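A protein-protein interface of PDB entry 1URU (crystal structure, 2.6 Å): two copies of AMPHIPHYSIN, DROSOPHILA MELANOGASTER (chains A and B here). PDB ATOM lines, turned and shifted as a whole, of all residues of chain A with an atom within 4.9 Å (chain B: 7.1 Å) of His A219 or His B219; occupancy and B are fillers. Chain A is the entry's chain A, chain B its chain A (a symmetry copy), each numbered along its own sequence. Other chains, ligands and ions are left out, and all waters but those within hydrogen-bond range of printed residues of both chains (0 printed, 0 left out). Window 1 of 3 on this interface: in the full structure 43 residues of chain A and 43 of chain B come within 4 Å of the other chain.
O of Phe A218 is in hydrogen-bond range of OG1 of Thr A222, 2.7 Å away. The side-chain hydroxyl (OH) of Tyr B63 sits at hydrogen-bond distance from the side-chain carboxylate (OE2) of Glu B215, at 2.5 Å. O of Phe B218 is in hydrogen-bond range of OG1 of Thr B222 (2.7 Å).
Printed residues of chain A that touch a printed residue of chain B: Glu A215, Gln A216, His A219, Asn A220, Thr A222, Ala A223 and Tyr A226. Hydrophobic or aromatic side chains of chain B that line the printed part of chain A: His B219, Ala B223 and Tyr B226.
Gln A216 touches Tyr B226, and with the chains exchanged Tyr A226 touches Gln B216. His B219 touches its own counterpart, His A219. His A219 touches Ala B223, and with the chains exchanged Ala A223 touches His B219. Asn A220 touches Ala B223, and with the chains exchanged Ala A223 touches Asn B220. Positions printed for both chains: 215, 216, 217, 218, 219, 220, 221, 222, 223 and 226. Of the 15 pairs that touch across the chains among the printed residues, 15 have their exchanged pair printed and touching as well.
Among the printed residues, pairs that only touch across the chains: Gln A216 with Tyr B226 (3.9 Å), His A219 with Thr B222 (3.7 Å), His A219 with Ala B223 (3.99 Å), His A219 with Tyr B226 (3.9 Å), Asn A220 with Ala B223 (3.8 Å), Thr A222 with His B219 (3.7 Å), Ala A223 with His B219 (3.99 Å), Ala A223 with Asn B220 (3.8 Å), Tyr A226 with Gln B216 (3.9 Å) and Tyr A226 with His B219 (3.9 Å).
OE2 of Glu A215 is in hydrogen-bond range of OH of Tyr B226. The side-chain amide oxygen (OE1) of Gln A216 lies close to the backbone carbonyl oxygen (O) of Ala B223. A ring nitrogen (ND1) of His A219 lies within hydrogen-bond range of a ring nitrogen (ND1) of His B219 (2.8 Å). OE1 of Gln B216 lies close to O of Ala A223 (3.1 Å). OH of Tyr A226 is in hydrogen-bond range of OE2 of Glu B215, at 3.4 Å.
Printed residues of chain B within 4 Å of Gln A216: Ala B223 (3.1 Å) and Tyr B226 (3.9 Å). Of the printed residues of chain B, His A219 touches His B219 (2.8 Å), Thr B222 (3.7 Å), Ala B223 (3.99 Å) and Tyr B226 (3.9 Å). Glu A221 touches none of the printed residues of chain B. Printed residues of chain A within 4 Å of His B219: His A219 (2.8 Å), Thr A222 (3.7 Å), Ala A223 (3.99 Å) and Tyr A226 (3.9 Å). Printed residues of chain A within 4 Å of Asn B220: Ala A223 (3.8 Å). Glu B221 touches none of the printed residues of chain A. The nearest printed residue of chain B that does not touch His A219 is Phe B218 (4.05 Å). The nearest printed residue of chain A that does not touch His B219 is Phe A218 (4.05 Å). The nearest printed residue of chain A that does not touch Ala B223 is Glu A215 (5.7 Å).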
ATOM      1  N   GLU A 215       7.636 -13.141  -3.309  1.00  0.00           N
ATOM      2  CA  GLU A 215       8.072 -13.817  -4.513  1.00  0.00           C
ATOM      3  C   GLU A 215       9.595 -13.783  -4.600  1.00  0.00           C
ATOM      4  O   GLU A 215      10.230 -14.800  -4.792  1.00  0.00           O
ATOM      5  CB  GLU A 215       7.464 -13.167  -5.749  1.00  0.00           C
ATOM      6  CG  GLU A 215       5.949 -13.249  -5.840  1.00  0.00           C
ATOM      7  CD  GLU A 215       5.436 -14.489  -6.558  1.00  0.00           C
ATOM      8  OE1 GLU A 215       6.137 -15.503  -6.645  1.00  0.00           O
ATOM      9  OE2 GLU A 215       4.296 -14.441  -7.038  1.00  0.00           O
ATOM     10  N   GLN A 216      10.178 -12.609  -4.423  1.00  0.00           N
ATOM     11  CA  GLN A 216      11.625 -12.440  -4.547  1.00  0.00           C
ATOM     12  C   GLN A 216      12.362 -13.382  -3.612  1.00  0.00           C
ATOM     13  O   GLN A 216      13.258 -14.102  -4.025  1.00  0.00           O
ATOM     14  CB  GLN A 216      12.025 -10.973  -4.272  1.00  0.00           C
ATOM     15  CG  GLN A 216      13.337 -10.727  -3.479  1.00  0.00           C
ATOM     16  CD  GLN A 216      14.577 -11.143  -4.235  1.00  0.00           C
ATOM     17  OE1 GLN A 216      14.730 -10.831  -5.415  1.00  0.00           O
ATOM     18  NE2 GLN A 216      15.471 -11.848  -3.557  1.00  0.00           N
ATOM     19  N   VAL A 217      11.972 -13.368  -2.345  1.00  0.00           N
ATOM     20  CA  VAL A 217      12.668 -14.141  -1.333  1.00  0.00           C
ATOM     21  C   VAL A 217      12.555 -15.629  -1.658  1.00  0.00           C
ATOM     22  O   VAL A 217      13.567 -16.315  -1.680  1.00  0.00           O
ATOM     23  CB  VAL A 217      12.149 -13.790   0.087  1.00  0.00           C
ATOM     24  CG1 VAL A 217      12.319 -14.948   1.059  1.00  0.00           C
ATOM     25  CG2 VAL A 217      12.856 -12.547   0.610  1.00  0.00           C
ATOM     26  N   PHE A 218      11.337 -16.107  -1.937  1.00  0.00           N
ATOM     27  CA  PHE A 218      11.087 -17.516  -2.301  1.00  0.00           C
ATOM     28  C   PHE A 218      11.910 -17.978  -3.494  1.00  0.00           C
ATOM     29  O   PHE A 218      12.507 -19.049  -3.476  1.00  0.00           O
ATOM     30  CB  PHE A 218       9.611 -17.720  -2.620  1.00  0.00           C
ATOM     31  CG  PHE A 218       9.317 -18.982  -3.363  1.00  0.00           C
ATOM     32  CD1 PHE A 218       9.358 -20.210  -2.716  1.00  0.00           C
ATOM     33  CD2 PHE A 218       8.979 -18.949  -4.713  1.00  0.00           C
ATOM     34  CE1 PHE A 218       9.073 -21.385  -3.397  1.00  0.00           C
ATOM     35  CE2 PHE A 218       8.685 -20.120  -5.406  1.00  0.00           C
ATOM     36  CZ  PHE A 218       8.739 -21.339  -4.744  1.00  0.00           C
ATOM     37  N   HIS A 219      11.956 -17.157  -4.532  1.00  0.00           N
ATOM     38  CA  HIS A 219      12.606 -17.552  -5.759  1.00  0.00           C
ATOM     39  C   HIS A 219      14.126 -17.547  -5.615  1.00  0.00           C
ATOM     40  O   HIS A 219      14.807 -18.389  -6.172  1.00  0.00           O
ATOM     41  CB  HIS A 219      12.133 -16.659  -6.905  1.00  0.00           C
ATOM     42  CG  HIS A 219      10.839 -17.103  -7.505  1.00  0.00           C
ATOM     43  ND1 HIS A 219      10.687 -18.331  -8.102  1.00  0.00           N
ATOM     44  CD2 HIS A 219       9.632 -16.492  -7.587  1.00  0.00           C
ATOM     45  CE1 HIS A 219       9.442 -18.457  -8.531  1.00  0.00           C
ATOM     46  NE2 HIS A 219       8.783 -17.347  -8.244  1.00  0.00           N
ATOM     47  N   ASN A 220      14.643 -16.609  -4.839  1.00  0.00           N
ATOM     48  CA  ASN A 220      16.069 -16.417  -4.695  1.00  0.00           C
ATOM     49  C   ASN A 220      16.669 -17.444  -3.741  1.00  0.00           C
ATOM     50  O   ASN A 220      17.770 -17.948  -3.966  1.00  0.00           O
ATOM     51  CB  ASN A 220      16.345 -15.010  -4.179  1.00  0.00           C
ATOM     52  CG  ASN A 220      17.786 -14.784  -3.869  1.00  0.00           C
ATOM     53  OD1 ASN A 220      18.132 -14.460  -2.750  1.00  0.00           O
ATOM     54  ND2 ASN A 220      18.652 -14.982  -4.862  1.00  0.00           N
ATOM     55  N   GLU A 221      15.949 -17.756  -2.667  1.00  0.00           N
ATOM     56  CA  GLU A 221      16.390 -18.819  -1.767  1.00  0.00           C
ATOM     57  C   GLU A 221      16.256 -20.166  -2.458  1.00  0.00           C
ATOM     58  O   GLU A 221      17.207 -20.919  -2.490  1.00  0.00           O
ATOM     59  CB  GLU A 221      15.621 -18.810  -0.439  1.00  0.00           C
ATOM     60  CG  GLU A 221      15.851 -17.595   0.461  1.00  0.00           C
ATOM     61  CD  GLU A 221      17.307 -17.212   0.607  1.00  0.00           C
ATOM     62  OE1 GLU A 221      18.161 -18.105   0.795  1.00  0.00           O
ATOM     63  OE2 GLU A 221      17.589 -15.997   0.503  1.00  0.00           O
ATOM     64  N   THR A 222      15.097 -20.456  -3.035  1.00  0.00           N
ATOM     65  CA  THR A 222      14.931 -21.682  -3.816  1.00  0.00           C
ATOM     66  C   THR A 222      16.021 -21.795  -4.884  1.00  0.00           C
ATOM     67  O   THR A 222      16.411 -22.891  -5.228  1.00  0.00           O
ATOM     68  CB  THR A 222      13.530 -21.762  -4.499  1.00  0.00           C
ATOM     69  OG1 THR A 222      12.479 -21.787  -3.537  1.00  0.00           O
ATOM     70  CG2 THR A 222      13.343 -23.081  -5.168  1.00  0.00           C
ATOM     71  N   ALA A 223      16.521 -20.681  -5.410  1.00  0.00           N
ATOM     72  CA  ALA A 223      17.592 -20.760  -6.415  1.00  0.00           C
ATOM     73  C   ALA A 223      18.907 -21.268  -5.808  1.00  0.00           C
ATOM     74  O   ALA A 223      19.553 -22.178  -6.341  1.00  0.00           O
ATOM     75  CB  ALA A 223      17.800 -19.430  -7.097  1.00  0.00           C
ATOM     76  N   TYR A 226      18.742 -25.037  -5.362  1.00  0.00           N
ATOM     77  CA  TYR A 226      18.882 -25.800  -6.589  1.00  0.00           C
ATOM     78  C   TYR A 226      20.317 -25.776  -7.121  1.00  0.00           C
ATOM     79  O   TYR A 226      20.701 -26.748  -7.747  1.00  0.00           O
ATOM     80  CB  TYR A 226      17.840 -25.392  -7.662  1.00  0.00           C
ATOM     81  CG  TYR A 226      16.508 -26.127  -7.511  1.00  0.00           C
ATOM     82  CD1 TYR A 226      15.305 -25.448  -7.276  1.00  0.00           C
ATOM     83  CD2 TYR A 226      16.460 -27.498  -7.570  1.00  0.00           C
ATOM     84  CE1 TYR A 226      14.091 -26.148  -7.123  1.00  0.00           C
ATOM     85  CE2 TYR A 226      15.283 -28.191  -7.423  1.00  0.00           C
ATOM     86  CZ  TYR A 226      14.103 -27.526  -7.205  1.00  0.00           C
ATOM     87  OH  TYR A 226      12.979 -28.284  -7.069  1.00  0.00           O
ATOM     88  N   TYR B  63       4.183 -33.031 -11.590  1.00  0.00           N
ATOM     89  CA  TYR B  63       4.872 -31.760 -11.390  1.00  0.00           C
ATOM     90  C   TYR B  63       4.714 -30.859 -12.591  1.00  0.00           C
ATOM     91  O   TYR B  63       4.448 -29.681 -12.447  1.00  0.00           O
ATOM     92  CB  TYR B  63       6.339 -32.009 -11.153  1.00  0.00           C
ATOM     93  CG  TYR B  63       7.166 -30.787 -10.860  1.00  0.00           C
ATOM     94  CD1 TYR B  63       6.938 -30.034  -9.718  1.00  0.00           C
ATOM     95  CD2 TYR B  63       8.208 -30.402 -11.704  1.00  0.00           C
ATOM     96  CE1 TYR B  63       7.717 -28.915  -9.412  1.00  0.00           C
ATOM     97  CE2 TYR B  63       8.997 -29.276 -11.413  1.00  0.00           C
ATOM     98  CZ  TYR B  63       8.743 -28.551 -10.250  1.00  0.00           C
ATOM     99  OH  TYR B  63       9.492 -27.465  -9.935  1.00  0.00           O
ATOM    100  N   LEU B 105      10.289 -16.579 -19.024  1.00  0.00           N
ATOM    101  CA  LEU B 105      11.032 -17.477 -18.141  1.00  0.00           C
ATOM    102  C   LEU B 105      10.161 -18.675 -17.796  1.00  0.00           C
ATOM    103  O   LEU B 105      10.628 -19.812 -17.801  1.00  0.00           O
ATOM    104  CB  LEU B 105      11.439 -16.797 -16.853  1.00  0.00           C
ATOM    105  CG  LEU B 105      12.439 -15.664 -16.992  1.00  0.00           C
ATOM    106  CD1 LEU B 105      12.569 -14.939 -15.665  1.00  0.00           C
ATOM    107  CD2 LEU B 105      13.786 -16.178 -17.429  1.00  0.00           C
ATOM    108  N   TRP B 106       8.897 -18.406 -17.485  1.00  0.00           N
ATOM    109  CA  TRP B 106       7.976 -19.470 -17.160  1.00  0.00           C
ATOM    110  C   TRP B 106       7.852 -20.410 -18.354  1.00  0.00           C
ATOM    111  O   TRP B 106       7.678 -21.613 -18.181  1.00  0.00           O
ATOM    112  CB  TRP B 106       6.591 -18.926 -16.798  1.00  0.00           C
ATOM    113  CG  TRP B 106       6.351 -18.610 -15.314  1.00  0.00           C
ATOM    114  CD1 TRP B 106       6.429 -17.377 -14.707  1.00  0.00           C
ATOM    115  CD2 TRP B 106       5.973 -19.534 -14.283  1.00  0.00           C
ATOM    116  NE1 TRP B 106       6.114 -17.487 -13.376  1.00  0.00           N
ATOM    117  CE2 TRP B 106       5.832 -18.794 -13.083  1.00  0.00           C
ATOM    118  CE3 TRP B 106       5.725 -20.915 -14.250  1.00  0.00           C
ATOM    119  CZ2 TRP B 106       5.451 -19.386 -11.867  1.00  0.00           C
ATOM    120  CZ3 TRP B 106       5.347 -21.506 -13.033  1.00  0.00           C
ATOM    121  CH2 TRP B 106       5.214 -20.739 -11.862  1.00  0.00           C
ATOM    122  N   PHE B 109      11.223 -22.605 -18.696  1.00  0.00           N
ATOM    123  CA  PHE B 109      11.062 -23.538 -17.587  1.00  0.00           C
ATOM    124  C   PHE B 109      10.163 -24.694 -18.000  1.00  0.00           C
ATOM    125  O   PHE B 109      10.589 -25.833 -17.979  1.00  0.00           O
ATOM    126  CB  PHE B 109      10.518 -22.794 -16.356  1.00  0.00           C
ATOM    127  CG  PHE B 109      10.409 -23.642 -15.106  1.00  0.00           C
ATOM    128  CD1 PHE B 109      11.498 -24.360 -14.628  1.00  0.00           C
ATOM    129  CD2 PHE B 109       9.207 -23.709 -14.398  1.00  0.00           C
ATOM    130  CE1 PHE B 109      11.386 -25.148 -13.464  1.00  0.00           C
ATOM    131  CE2 PHE B 109       9.087 -24.475 -13.249  1.00  0.00           C
ATOM    132  CZ  PHE B 109      10.166 -25.199 -12.781  1.00  0.00           C
ATOM    133  N   ALA B 213      19.321 -27.738 -12.900  1.00  0.00           N
ATOM    134  CA  ALA B 213      19.798 -26.567 -13.622  1.00  0.00           C
ATOM    135  C   ALA B 213      18.643 -25.760 -14.215  1.00  0.00           C
ATOM    136  O   ALA B 213      18.711 -24.533 -14.329  1.00  0.00           O
ATOM    137  CB  ALA B 213      20.719 -27.029 -14.748  1.00  0.00           C
ATOM    138  N   THR B 214      17.599 -26.465 -14.636  1.00  0.00           N
ATOM    139  CA  THR B 214      16.438 -25.846 -15.235  1.00  0.00           C
ATOM    140  C   THR B 214      15.743 -25.056 -14.163  1.00  0.00           C
ATOM    141  O   THR B 214      15.369 -23.890 -14.380  1.00  0.00           O
ATOM    142  CB  THR B 214      15.508 -26.939 -15.795  1.00  0.00           C
ATOM    143  OG1 THR B 214      16.203 -27.663 -16.814  1.00  0.00           O
ATOM    144  CG2 THR B 214      14.293 -26.371 -16.493  1.00  0.00           C
ATOM    145  N   GLU B 215      15.613 -25.706 -13.002  1.00  0.00           N
ATOM    146  CA  GLU B 215      15.035 -25.103 -11.819  1.00  0.00           C
ATOM    147  C   GLU B 215      15.873 -23.900 -11.393  1.00  0.00           C
ATOM    148  O   GLU B 215      15.353 -22.823 -11.184  1.00  0.00           O
ATOM    149  CB  GLU B 215      14.958 -26.113 -10.681  1.00  0.00           C
ATOM    150  CG  GLU B 215      14.047 -27.302 -10.938  1.00  0.00           C
ATOM    151  CD  GLU B 215      12.605 -27.087 -10.500  1.00  0.00           C
ATOM    152  OE1 GLU B 215      12.147 -25.946 -10.378  1.00  0.00           O
ATOM    153  OE2 GLU B 215      11.918 -28.093 -10.282  1.00  0.00           O
ATOM    154  N   GLN B 216      17.179 -24.084 -11.298  1.00  0.00           N
ATOM    155  CA  GLN B 216      18.076 -23.024 -10.839  1.00  0.00           C
ATOM    156  C   GLN B 216      17.921 -21.777 -11.690  1.00  0.00           C
ATOM    157  O   GLN B 216      17.735 -20.685 -11.176  1.00  0.00           O
ATOM    158  CB  GLN B 216      19.542 -23.514 -10.846  1.00  0.00           C
ATOM    159  CG  GLN B 216      20.631 -22.501 -11.295  1.00  0.00           C
ATOM    160  CD  GLN B 216      20.800 -21.346 -10.337  1.00  0.00           C
ATOM    161  OE1 GLN B 216      20.875 -21.539  -9.123  1.00  0.00           O
ATOM    162  NE2 GLN B 216      20.866 -20.138 -10.877  1.00  0.00           N
ATOM    163  N   VAL B 217      18.000 -21.954 -13.002  1.00  0.00           N
ATOM    164  CA  VAL B 217      17.978 -20.828 -13.917  1.00  0.00           C
ATOM    165  C   VAL B 217      16.640 -20.100 -13.800  1.00  0.00           C
ATOM    166  O   VAL B 217      16.631 -18.888 -13.635  1.00  0.00           O
ATOM    167  CB  VAL B 217      18.294 -21.285 -15.367  1.00  0.00           C
ATOM    168  CG1 VAL B 217      17.664 -20.368 -16.405  1.00  0.00           C
ATOM    169  CG2 VAL B 217      19.801 -21.368 -15.573  1.00  0.00           C
ATOM    170  N   PHE B 218      15.529 -20.843 -13.855  1.00  0.00           N
ATOM    171  CA  PHE B 218      14.172 -20.277 -13.722  1.00  0.00           C
ATOM    172  C   PHE B 218      13.982 -19.483 -12.438  1.00  0.00           C
ATOM    173  O   PHE B 218      13.443 -18.380 -12.448  1.00  0.00           O
ATOM    174  CB  PHE B 218      13.133 -21.391 -13.764  1.00  0.00           C
ATOM    175  CG  PHE B 218      11.787 -20.988 -13.255  1.00  0.00           C
ATOM    176  CD1 PHE B 218      10.959 -20.173 -14.016  1.00  0.00           C
ATOM    177  CD2 PHE B 218      11.331 -21.437 -12.019  1.00  0.00           C
ATOM    178  CE1 PHE B 218       9.703 -19.806 -13.556  1.00  0.00           C
ATOM    179  CE2 PHE B 218      10.070 -21.081 -11.550  1.00  0.00           C
ATOM    180  CZ  PHE B 218       9.259 -20.260 -12.320  1.00  0.00           C
ATOM    181  N   HIS B 219      14.441 -20.039 -11.328  1.00  0.00           N
ATOM    182  CA  HIS B 219      14.203 -19.428 -10.041  1.00  0.00           C
ATOM    183  C   HIS B 219      15.067 -18.183  -9.844  1.00  0.00           C
ATOM    184  O   HIS B 219      14.631 -17.213  -9.251  1.00  0.00           O
ATOM    185  CB  HIS B 219      14.415 -20.457  -8.933  1.00  0.00           C
ATOM    186  CG  HIS B 219      13.219 -21.319  -8.690  1.00  0.00           C
ATOM    187  ND1 HIS B 219      12.011 -20.804  -8.288  1.00  0.00           N
ATOM    188  CD2 HIS B 219      13.039 -22.657  -8.807  1.00  0.00           C
ATOM    189  CE1 HIS B 219      11.136 -21.790  -8.163  1.00  0.00           C
ATOM    190  NE2 HIS B 219      11.739 -22.928  -8.459  1.00  0.00           N
ATOM    191  N   ASN B 220      16.279 -18.216 -10.371  1.00  0.00           N
ATOM    192  CA  ASN B 220      17.242 -17.155 -10.173  1.00  0.00           C
ATOM    193  C   ASN B 220      16.948 -15.967 -11.084  1.00  0.00           C
ATOM    194  O   ASN B 220      17.090 -14.812 -10.680  1.00  0.00           O
ATOM    195  CB  ASN B 220      18.644 -17.682 -10.448  1.00  0.00           C
ATOM    196  CG  ASN B 220      19.680 -16.609 -10.404  1.00  0.00           C
ATOM    197  OD1 ASN B 220      20.378 -16.387 -11.372  1.00  0.00           O
ATOM    198  ND2 ASN B 220      19.770 -15.910  -9.273  1.00  0.00           N
ATOM    199  N   GLU B 221      16.542 -16.245 -12.319  1.00  0.00           N
ATOM    200  CA  GLU B 221      16.120 -15.173 -13.216  1.00  0.00           C
ATOM    201  C   GLU B 221      14.805 -14.585 -12.733  1.00  0.00           C
ATOM    202  O   GLU B 221      14.705 -13.386 -12.578  1.00  0.00           O
ATOM    203  CB  GLU B 221      16.004 -15.647 -14.671  1.00  0.00           C
ATOM    204  CG  GLU B 221      17.312 -16.054 -15.350  1.00  0.00           C
ATOM    205  CD  GLU B 221      18.446 -15.080 -15.125  1.00  0.00           C
ATOM    206  OE1 GLU B 221      18.229 -13.853 -15.221  1.00  0.00           O
ATOM    207  OE2 GLU B 221      19.560 -15.564 -14.821  1.00  0.00           O
ATOM    208  N   THR B 222      13.812 -15.424 -12.464  1.00  0.00           N
ATOM    209  CA  THR B 222      12.556 -14.943 -11.887  1.00  0.00           C
ATOM    210  C   THR B 222      12.821 -14.119 -10.626  1.00  0.00           C
ATOM    211  O   THR B 222      12.070 -13.212 -10.332  1.00  0.00           O
ATOM    212  CB  THR B 222      11.577 -16.110 -11.546  1.00  0.00           C
ATOM    213  OG1 THR B 222      11.199 -16.834 -12.712  1.00  0.00           O
ATOM    214  CG2 THR B 222      10.260 -15.579 -11.093  1.00  0.00           C
ATOM    215  N   ALA B 223      13.879 -14.417  -9.875  1.00  0.00           N
ATOM    216  CA  ALA B 223      14.175 -13.621  -8.675  1.00  0.00           C
ATOM    217  C   ALA B 223      14.613 -12.195  -9.030  1.00  0.00           C
ATOM    218  O   ALA B 223      14.110 -11.209  -8.477  1.00  0.00           O
ATOM    219  CB  ALA B 223      15.213 -14.299  -7.814  1.00  0.00           C
ATOM    220  N   LYS B 224      15.559 -12.106  -9.961  1.00  0.00           N
ATOM    221  CA  LYS B 224      15.996 -10.832 -10.536  1.00  0.00           C
ATOM    222  C   LYS B 224      14.819  -9.981 -11.029  1.00  0.00           C
ATOM    223  O   LYS B 224      14.873  -8.773 -10.942  1.00  0.00           O
ATOM    224  CB  LYS B 224      16.979 -11.058 -11.699  1.00  0.00           C
ATOM    225  CG  LYS B 224      18.372 -11.537 -11.290  1.00  0.00           C
ATOM    226  CD  LYS B 224      19.315 -11.622 -12.509  1.00  0.00           C
ATOM    227  CE  LYS B 224      20.464 -12.618 -12.264  1.00  0.00           C
ATOM    228  NZ  LYS B 224      21.103 -13.081 -13.545  1.00  0.00           N
ATOM    229  N   ILE B 225      13.774 -10.611 -11.548  1.00  0.00           N
ATOM    230  CA  ILE B 225      12.621  -9.890 -12.074  1.00  0.00           C
ATOM    231  C   ILE B 225      11.808  -9.289 -10.955  1.00  0.00           C
ATOM    232  O   ILE B 225      11.372  -8.136 -11.033  1.00  0.00           O
ATOM    233  CB  ILE B 225      11.715 -10.844 -12.816  1.00  0.00           C
ATOM    234  CG1 ILE B 225      12.381 -11.285 -14.110  1.00  0.00           C
ATOM    235  CG2 ILE B 225      10.307 -10.209 -13.009  1.00  0.00           C
ATOM    236  CD1 ILE B 225      11.419 -11.471 -15.276  1.00  0.00           C
ATOM    237  N   TYR B 226      11.571 -10.106  -9.936  1.00  0.00           N
ATOM    238  CA  TYR B 226      10.759  -9.695  -8.806  1.00  0.00           C
ATOM    239  C   TYR B 226      11.440  -8.610  -7.970  1.00  0.00           C
ATOM    240  O   TYR B 226      10.724  -7.813  -7.391  1.00  0.00           O
ATOM    241  CB  TYR B 226      10.284 -10.899  -7.950  1.00  0.00           C
ATOM    242  CG  TYR B 226       8.998 -11.536  -8.477  1.00  0.00           C
ATOM    243  CD1 TYR B 226       8.946 -12.874  -8.891  1.00  0.00           C
ATOM    244  CD2 TYR B 226       7.849 -10.792  -8.589  1.00  0.00           C
ATOM    245  CE1 TYR B 226       7.752 -13.435  -9.390  1.00  0.00           C
ATOM    246  CE2 TYR B 226       6.680 -11.329  -9.073  1.00  0.00           C
ATOM    247  CZ  TYR B 226       6.625 -12.642  -9.467  1.00  0.00           C
ATOM    248  OH  TYR B 226       5.431 -13.098  -9.936  1.00  0.00           O
